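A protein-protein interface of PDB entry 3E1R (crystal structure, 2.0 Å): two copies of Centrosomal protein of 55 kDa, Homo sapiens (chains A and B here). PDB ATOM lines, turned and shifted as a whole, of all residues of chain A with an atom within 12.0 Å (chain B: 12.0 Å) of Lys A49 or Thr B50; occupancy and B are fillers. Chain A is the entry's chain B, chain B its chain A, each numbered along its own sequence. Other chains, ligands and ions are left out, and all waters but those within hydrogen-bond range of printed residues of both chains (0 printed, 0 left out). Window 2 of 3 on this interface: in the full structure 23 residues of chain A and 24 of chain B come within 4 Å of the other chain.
The side-chain amino group (NZ) of Lys B42 is in salt-bridge range of the side-chain carboxylate (OE2) of Glu B45.
O of Leu B46 lies within hydrogen-bond range of OG1 of Thr B50.
The side-chain amino group (NZ) of Lys A49 lies within salt-bridge range of the side-chain carboxylate (OE1) of Glu A45 (2.7 Å).
Along chain B the printed residues that touch a printed residue of chain A span positions 42 to 50.
Printed residues of chain A that touch a printed residue of chain B: Lys A42, Ile A43, Leu A46, Glu A47 and Lys A49.
Among the printed residues, 7 pairs touch across the chains.
Among the printed residues, no Asp or Glu carboxylate lies within 4 Å of a Lys or Arg side-chain nitrogen of the other chain.
Lys A42 touches Ile B43 (CD to CD1, 3.9 Å).
Ile A43 touches Ile B43 (CG1 to CG1, 3.5 Å).
CB of Leu A46 touches CG of Leu B46, at 3.9 Å.
Leu A46 touches Glu B47.
OG1 of Thr B50 touches CD2 of Leu A46, at 3.7 Å.
OE2 of Glu A47 touches CE of Lys B42, at 3.5 Å.
Thr B50 touches Lys A49.
Thr B50 touches just these residues of chain A: Leu A46 and Lys A49.
No residue of chain B comes within 4 Å of Glu A45.
Leu A46 touches three residues of chain B.
Of chain A, only Leu A46 (3.9 Å) comes within 4 Å of Leu B46.
No residue of chain A comes within 4 Å of Lys B49.
No residue of chain A comes within 4 Å of Glu B51.
Of the printed residues of chain B, Ile A43 touches Ile B43 (3.5 Å).
Printed residues of chain B within 4 Å of Lys A42: Ile B43 (3.9 Å).
Of the printed residues of chain B, Glu A47 touches Lys B42.
Of the printed residues of chain A, Ile B43 touches Lys A42 and Ile A43.
Of the printed residues of chain A, Lys B42 touches Glu A47 (3.5 Å).
The nearest residue of chain B that does not touch Lys A49 is Lys B49 (6.5 Å).
The nearest residue of chain A that does not touch Thr B50 is Glu A47 (6.1 Å).
The nearest printed residue of chain B that does not touch Ile A43 is Lys B42 (4.03 Å).
Lys A42 touches Ile B43, but with the chains exchanged Ile A43 does not touch Lys B42 (4.03 Å).
Leu B46 touches its own counterpart, Leu A46.
Leu A46 touches Glu B47, but with the chains exchanged Glu A47 does not touch Leu B46 (4.1 Å).
Glu A47 touches Lys B42, but with the chains exchanged Lys A42 does not touch Glu B47 (4.3 Å).
9 positions are printed for both chains.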
ATOM      1  N   LEU A  40     -13.165  29.684  16.448  1.00  0.00           N
ATOM      2  CA  LEU A  40     -13.849  28.512  15.900  1.00  0.00           C
ATOM      3  C   LEU A  40     -14.052  27.429  16.966  1.00  0.00           C
ATOM      4  O   LEU A  40     -15.070  26.737  16.970  1.00  0.00           O
ATOM      5  CB  LEU A  40     -13.061  27.920  14.723  1.00  0.00           C
ATOM      6  CG  LEU A  40     -13.060  28.745  13.436  1.00  0.00           C
ATOM      7  CD1 LEU A  40     -11.984  28.234  12.479  1.00  0.00           C
ATOM      8  CD2 LEU A  40     -14.444  28.681  12.804  1.00  0.00           C
ATOM      9  N   ALA A  41     -13.083  27.281  17.862  1.00  0.00           N
ATOM     10  CA  ALA A  41     -13.167  26.281  18.921  1.00  0.00           C
ATOM     11  C   ALA A  41     -14.261  26.674  19.906  1.00  0.00           C
ATOM     12  O   ALA A  41     -15.001  25.824  20.395  1.00  0.00           O
ATOM     13  CB  ALA A  41     -11.818  26.149  19.642  1.00  0.00           C
ATOM     14  N   LYS A  42     -14.354  27.968  20.195  1.00  0.00           N
ATOM     15  CA  LYS A  42     -15.370  28.467  21.114  1.00  0.00           C
ATOM     16  C   LYS A  42     -16.757  28.193  20.515  1.00  0.00           C
ATOM     17  O   LYS A  42     -17.673  27.761  21.212  1.00  0.00           O
ATOM     18  CB  LYS A  42     -15.157  29.965  21.364  1.00  0.00           C
ATOM     19  CG  LYS A  42     -16.068  30.539  22.428  1.00  0.00           C
ATOM     20  CD  LYS A  42     -15.902  32.048  22.596  1.00  0.00           C
ATOM     21  CE  LYS A  42     -14.683  32.412  23.429  1.00  0.00           C
ATOM     22  NZ  LYS A  42     -14.862  33.760  24.047  1.00  0.00           N
ATOM     23  N   ILE A  43     -16.911  28.424  19.217  1.00  0.00           N
ATOM     24  CA  ILE A  43     -18.193  28.156  18.571  1.00  0.00           C
ATOM     25  C   ILE A  43     -18.557  26.668  18.652  1.00  0.00           C
ATOM     26  O   ILE A  43     -19.713  26.323  18.882  1.00  0.00           O
ATOM     27  CB  ILE A  43     -18.173  28.595  17.087  1.00  0.00           C
ATOM     28  CG1 ILE A  43     -18.242  30.120  17.002  1.00  0.00           C
ATOM     29  CG2 ILE A  43     -19.325  27.955  16.324  1.00  0.00           C
ATOM     30  CD1 ILE A  43     -17.873  30.687  15.635  1.00  0.00           C
ATOM     31  N   PHE A  44     -17.569  25.798  18.460  1.00  0.00           N
ATOM     32  CA  PHE A  44     -17.798  24.353  18.521  1.00  0.00           C
ATOM     33  C   PHE A  44     -18.309  23.971  19.902  1.00  0.00           C
ATOM     34  O   PHE A  44     -19.238  23.172  20.040  1.00  0.00           O
ATOM     35  CB  PHE A  44     -16.502  23.582  18.239  1.00  0.00           C
ATOM     36  CG  PHE A  44     -16.654  22.085  18.327  1.00  0.00           C
ATOM     37  CD1 PHE A  44     -17.282  21.367  17.314  1.00  0.00           C
ATOM     38  CD2 PHE A  44     -16.205  21.398  19.449  1.00  0.00           C
ATOM     39  CE1 PHE A  44     -17.444  19.980  17.410  1.00  0.00           C
ATOM     40  CE2 PHE A  44     -16.359  20.016  19.556  1.00  0.00           C
ATOM     41  CZ  PHE A  44     -16.988  19.306  18.538  1.00  0.00           C
ATOM     42  N   GLU A  45     -17.678  24.541  20.922  1.00  0.00           N
ATOM     43  CA  GLU A  45     -18.042  24.284  22.310  1.00  0.00           C
ATOM     44  C   GLU A  45     -19.464  24.780  22.600  1.00  0.00           C
ATOM     45  O   GLU A  45     -20.278  24.052  23.170  1.00  0.00           O
ATOM     46  CB  GLU A  45     -17.036  24.973  23.242  1.00  0.00           C
ATOM     47  CG  GLU A  45     -17.333  24.808  24.725  1.00  0.00           C
ATOM     48  CD  GLU A  45     -17.360  23.354  25.172  1.00  0.00           C
ATOM     49  OE1 GLU A  45     -18.233  23.005  25.995  1.00  0.00           O
ATOM     50  OE2 GLU A  45     -16.509  22.563  24.714  1.00  0.00           O
ATOM     51  N   LEU A  46     -19.763  26.009  22.189  1.00  0.00           N
ATOM     52  CA  LEU A  46     -21.088  26.584  22.404  1.00  0.00           C
ATOM     53  C   LEU A  46     -22.169  25.784  21.685  1.00  0.00           C
ATOM     54  O   LEU A  46     -23.291  25.674  22.177  1.00  0.00           O
ATOM     55  CB  LEU A  46     -21.113  28.048  21.949  1.00  0.00           C
ATOM     56  CG  LEU A  46     -20.469  29.049  22.922  1.00  0.00           C
ATOM     57  CD1 LEU A  46     -20.008  30.297  22.178  1.00  0.00           C
ATOM     58  CD2 LEU A  46     -21.473  29.405  24.014  1.00  0.00           C
ATOM     59  N   GLU A  47     -21.837  25.224  20.526  1.00  0.00           N
ATOM     60  CA  GLU A  47     -22.799  24.420  19.776  1.00  0.00           C
ATOM     61  C   GLU A  47     -23.084  23.099  20.506  1.00  0.00           C
ATOM     62  O   GLU A  47     -24.166  22.534  20.358  1.00  0.00           O
ATOM     63  CB  GLU A  47     -22.281  24.130  18.360  1.00  0.00           C
ATOM     64  CG  GLU A  47     -22.144  25.366  17.460  1.00  0.00           C
ATOM     65  CD  GLU A  47     -23.409  25.695  16.682  1.00  0.00           C
ATOM     66  OE1 GLU A  47     -24.504  25.259  17.097  1.00  0.00           O
ATOM     67  OE2 GLU A  47     -23.308  26.403  15.654  1.00  0.00           O
ATOM     68  N   LYS A  48     -22.121  22.605  21.285  1.00  0.00           N
ATOM     69  CA  LYS A  48     -22.321  21.361  22.031  1.00  0.00           C
ATOM     70  C   LYS A  48     -23.484  21.490  23.005  1.00  0.00           C
ATOM     71  O   LYS A  48     -24.186  20.517  23.274  1.00  0.00           O
ATOM     72  CB  LYS A  48     -21.078  20.972  22.837  1.00  0.00           C
ATOM     73  CG  LYS A  48     -20.054  20.109  22.128  1.00  0.00           C
ATOM     74  CD  LYS A  48     -19.253  19.343  23.172  1.00  0.00           C
ATOM     75  CE  LYS A  48     -17.885  18.924  22.677  1.00  0.00           C
ATOM     76  NZ  LYS A  48     -17.242  17.982  23.641  1.00  0.00           N
ATOM     77  N   LYS A  49     -23.679  22.686  23.556  1.00  0.00           N
ATOM     78  CA  LYS A  49     -24.766  22.911  24.500  1.00  0.00           C
ATOM     79  C   LYS A  49     -26.087  22.830  23.734  1.00  0.00           C
ATOM     80  O   LYS A  49     -26.872  23.799  23.814  1.00  0.00           O
ATOM     81  CB  LYS A  49     -24.655  24.292  25.155  1.00  0.00           C
ATOM     82  CG  LYS A  49     -23.239  24.760  25.488  1.00  0.00           C
ATOM     83  CD  LYS A  49     -22.522  23.851  26.472  1.00  0.00           C
ATOM     84  CE  LYS A  49     -21.182  24.456  26.868  1.00  0.00           C
ATOM     85  NZ  LYS A  49     -20.340  23.518  27.660  1.00  0.00           N
ATOM     86  N   ALA B  41     -20.015  37.328  15.495  1.00  0.00           N
ATOM     87  CA  ALA B  41     -21.469  37.470  15.534  1.00  0.00           C
ATOM     88  C   ALA B  41     -22.090  36.139  15.958  1.00  0.00           C
ATOM     89  O   ALA B  41     -23.038  36.105  16.742  1.00  0.00           O
ATOM     90  CB  ALA B  41     -22.003  37.889  14.165  1.00  0.00           C
ATOM     91  N   LYS B  42     -21.546  35.040  15.442  1.00  0.00           N
ATOM     92  CA  LYS B  42     -22.056  33.714  15.774  1.00  0.00           C
ATOM     93  C   LYS B  42     -21.875  33.430  17.258  1.00  0.00           C
ATOM     94  O   LYS B  42     -22.763  32.878  17.901  1.00  0.00           O
ATOM     95  CB  LYS B  42     -21.336  32.637  14.957  1.00  0.00           C
ATOM     96  CG  LYS B  42     -21.893  31.238  15.155  1.00  0.00           C
ATOM     97  CD  LYS B  42     -23.358  31.175  14.744  1.00  0.00           C
ATOM     98  CE  LYS B  42     -23.862  29.745  14.703  1.00  0.00           C
ATOM     99  NZ  LYS B  42     -25.203  29.651  14.063  1.00  0.00           N
ATOM    100  N   ILE B  43     -20.716  33.804  17.800  1.00  0.00           N
ATOM    101  CA  ILE B  43     -20.423  33.591  19.213  1.00  0.00           C
ATOM    102  C   ILE B  43     -21.391  34.382  20.096  1.00  0.00           C
ATOM    103  O   ILE B  43     -21.914  33.852  21.082  1.00  0.00           O
ATOM    104  CB  ILE B  43     -18.973  34.024  19.549  1.00  0.00           C
ATOM    105  CG1 ILE B  43     -17.977  32.981  19.026  1.00  0.00           C
ATOM    106  CG2 ILE B  43     -18.813  34.214  21.056  1.00  0.00           C
ATOM    107  CD1 ILE B  43     -16.535  33.462  19.011  1.00  0.00           C
ATOM    108  N   PHE B  44     -21.622  35.646  19.749  1.00  0.00           N
ATOM    109  CA  PHE B  44     -22.532  36.499  20.509  1.00  0.00           C
ATOM    110  C   PHE B  44     -23.929  35.875  20.526  1.00  0.00           C
ATOM    111  O   PHE B  44     -24.540  35.735  21.587  1.00  0.00           O
ATOM    112  CB  PHE B  44     -22.585  37.904  19.886  1.00  0.00           C
ATOM    113  CG  PHE B  44     -23.571  38.840  20.553  1.00  0.00           C
ATOM    114  CD1 PHE B  44     -23.284  39.425  21.782  1.00  0.00           C
ATOM    115  CD2 PHE B  44     -24.793  39.121  19.950  1.00  0.00           C
ATOM    116  CE1 PHE B  44     -24.202  40.285  22.402  1.00  0.00           C
ATOM    117  CE2 PHE B  44     -25.719  39.979  20.560  1.00  0.00           C
ATOM    118  CZ  PHE B  44     -25.423  40.557  21.785  1.00  0.00           C
ATOM    119  N   GLU B  45     -24.426  35.504  19.351  1.00  0.00           N
ATOM    120  CA  GLU B  45     -25.746  34.881  19.221  1.00  0.00           C
ATOM    121  C   GLU B  45     -25.858  33.615  20.068  1.00  0.00           C
ATOM    122  O   GLU B  45     -26.831  33.419  20.794  1.00  0.00           O
ATOM    123  CB  GLU B  45     -26.029  34.532  17.750  1.00  0.00           C
ATOM    124  CG  GLU B  45     -27.145  33.499  17.568  1.00  0.00           C
ATOM    125  CD  GLU B  45     -27.471  33.201  16.110  1.00  0.00           C
ATOM    126  OE1 GLU B  45     -28.032  34.088  15.428  1.00  0.00           O
ATOM    127  OE2 GLU B  45     -27.167  32.079  15.647  1.00  0.00           O
ATOM    128  N   LEU B  46     -24.857  32.749  19.965  1.00  0.00           N
ATOM    129  CA  LEU B  46     -24.841  31.497  20.710  1.00  0.00           C
ATOM    130  C   LEU B  46     -24.787  31.713  22.229  1.00  0.00           C
ATOM    131  O   LEU B  46     -25.444  30.996  22.987  1.00  0.00           O
ATOM    132  CB  LEU B  46     -23.641  30.653  20.256  1.00  0.00           C
ATOM    133  CG  LEU B  46     -23.742  29.378  19.412  1.00  0.00           C
ATOM    134  CD1 LEU B  46     -25.048  29.268  18.643  1.00  0.00           C
ATOM    135  CD2 LEU B  46     -22.539  29.367  18.473  1.00  0.00           C
ATOM    136  N   GLU B  47     -23.992  32.690  22.668  1.00  0.00           N
ATOM    137  CA  GLU B  47     -23.853  32.981  24.092  1.00  0.00           C
ATOM    138  C   GLU B  47     -25.151  33.472  24.724  1.00  0.00           C
ATOM    139  O   GLU B  47     -25.415  33.198  25.896  1.00  0.00           O
ATOM    140  CB  GLU B  47     -22.746  34.006  24.334  1.00  0.00           C
ATOM    141  CG  GLU B  47     -21.338  33.477  24.090  1.00  0.00           C
ATOM    142  CD  GLU B  47     -20.281  34.560  24.198  1.00  0.00           C
ATOM    143  OE1 GLU B  47     -20.599  35.736  23.927  1.00  0.00           O
ATOM    144  OE2 GLU B  47     -19.128  34.236  24.538  1.00  0.00           O
ATOM    145  N   LYS B  48     -25.955  34.207  23.969  1.00  0.00           N
ATOM    146  CA  LYS B  48     -27.214  34.669  24.532  1.00  0.00           C
ATOM    147  C   LYS B  48     -28.234  33.529  24.441  1.00  0.00           C
ATOM    148  O   LYS B  48     -29.086  33.387  25.313  1.00  0.00           O
ATOM    149  CB  LYS B  48     -27.704  35.947  23.827  1.00  0.00           C
ATOM    150  CG  LYS B  48     -27.967  35.872  22.338  1.00  0.00           C
ATOM    151  CD  LYS B  48     -28.279  37.277  21.806  1.00  0.00           C
ATOM    152  CE  LYS B  48     -29.264  37.242  20.648  1.00  0.00           C
ATOM    153  NZ  LYS B  48     -28.727  37.872  19.407  1.00  0.00           N
ATOM    154  N   LYS B  49     -28.113  32.697  23.407  1.00  0.00           N
ATOM    155  CA  LYS B  49     -29.012  31.558  23.232  1.00  0.00           C
ATOM    156  C   LYS B  49     -28.820  30.545  24.366  1.00  0.00           C
ATOM    157  O   LYS B  49     -29.793  30.038  24.916  1.00  0.00           O
ATOM    158  CB  LYS B  49     -28.778  30.880  21.867  1.00  0.00           C
ATOM    159  CG  LYS B  49     -29.665  29.652  21.604  1.00  0.00           C
ATOM    160  CD  LYS B  49     -29.757  29.282  20.112  1.00  0.00           C
ATOM    161  CE  LYS B  49     -28.548  28.494  19.609  1.00  0.00           C
ATOM    162  NZ  LYS B  49     -28.559  28.325  18.120  1.00  0.00           N
ATOM    163  N   THR B  50     -27.568  30.260  24.724  1.00  0.00           N
ATOM    164  CA  THR B  50     -27.280  29.303  25.795  1.00  0.00           C
ATOM    165  C   THR B  50     -27.298  29.944  27.187  1.00  0.00           C
ATOM    166  O   THR B  50     -27.376  29.240  28.197  1.00  0.00           O
ATOM    167  CB  THR B  50     -25.908  28.597  25.580  1.00  0.00           C
ATOM    168  OG1 THR B  50     -24.850  29.558  25.632  1.00  0.00           O
ATOM    169  CG2 THR B  50     -25.876  27.886  24.230  1.00  0.00           C
ATOM    170  N   GLU B  51     -27.222  31.274  27.226  1.00  0.00           N
ATOM    171  CA  GLU B  51     -27.256  32.064  28.462  1.00  0.00           C
ATOM    172  C   GLU B  51     -25.984  32.098  29.311  1.00  0.00           C
ATOM    173  O   GLU B  51     -26.007  31.588  30.453  1.00  0.00           O
ATOM    174  CB  GLU B  51     -28.459  31.650  29.319  1.00  0.00           C
ATOM    175  CG  GLU B  51     -29.788  31.918  28.616  1.00  0.00           C
ATOM    176  CD  GLU B  51     -30.985  31.919  29.551  1.00  0.00           C
ATOM    177  OE1 GLU B  51     -30.915  32.572  30.614  1.00  0.00           O
ATOM    178  OE2 GLU B  51     -32.004  31.282  29.211  1.00  0.00           O
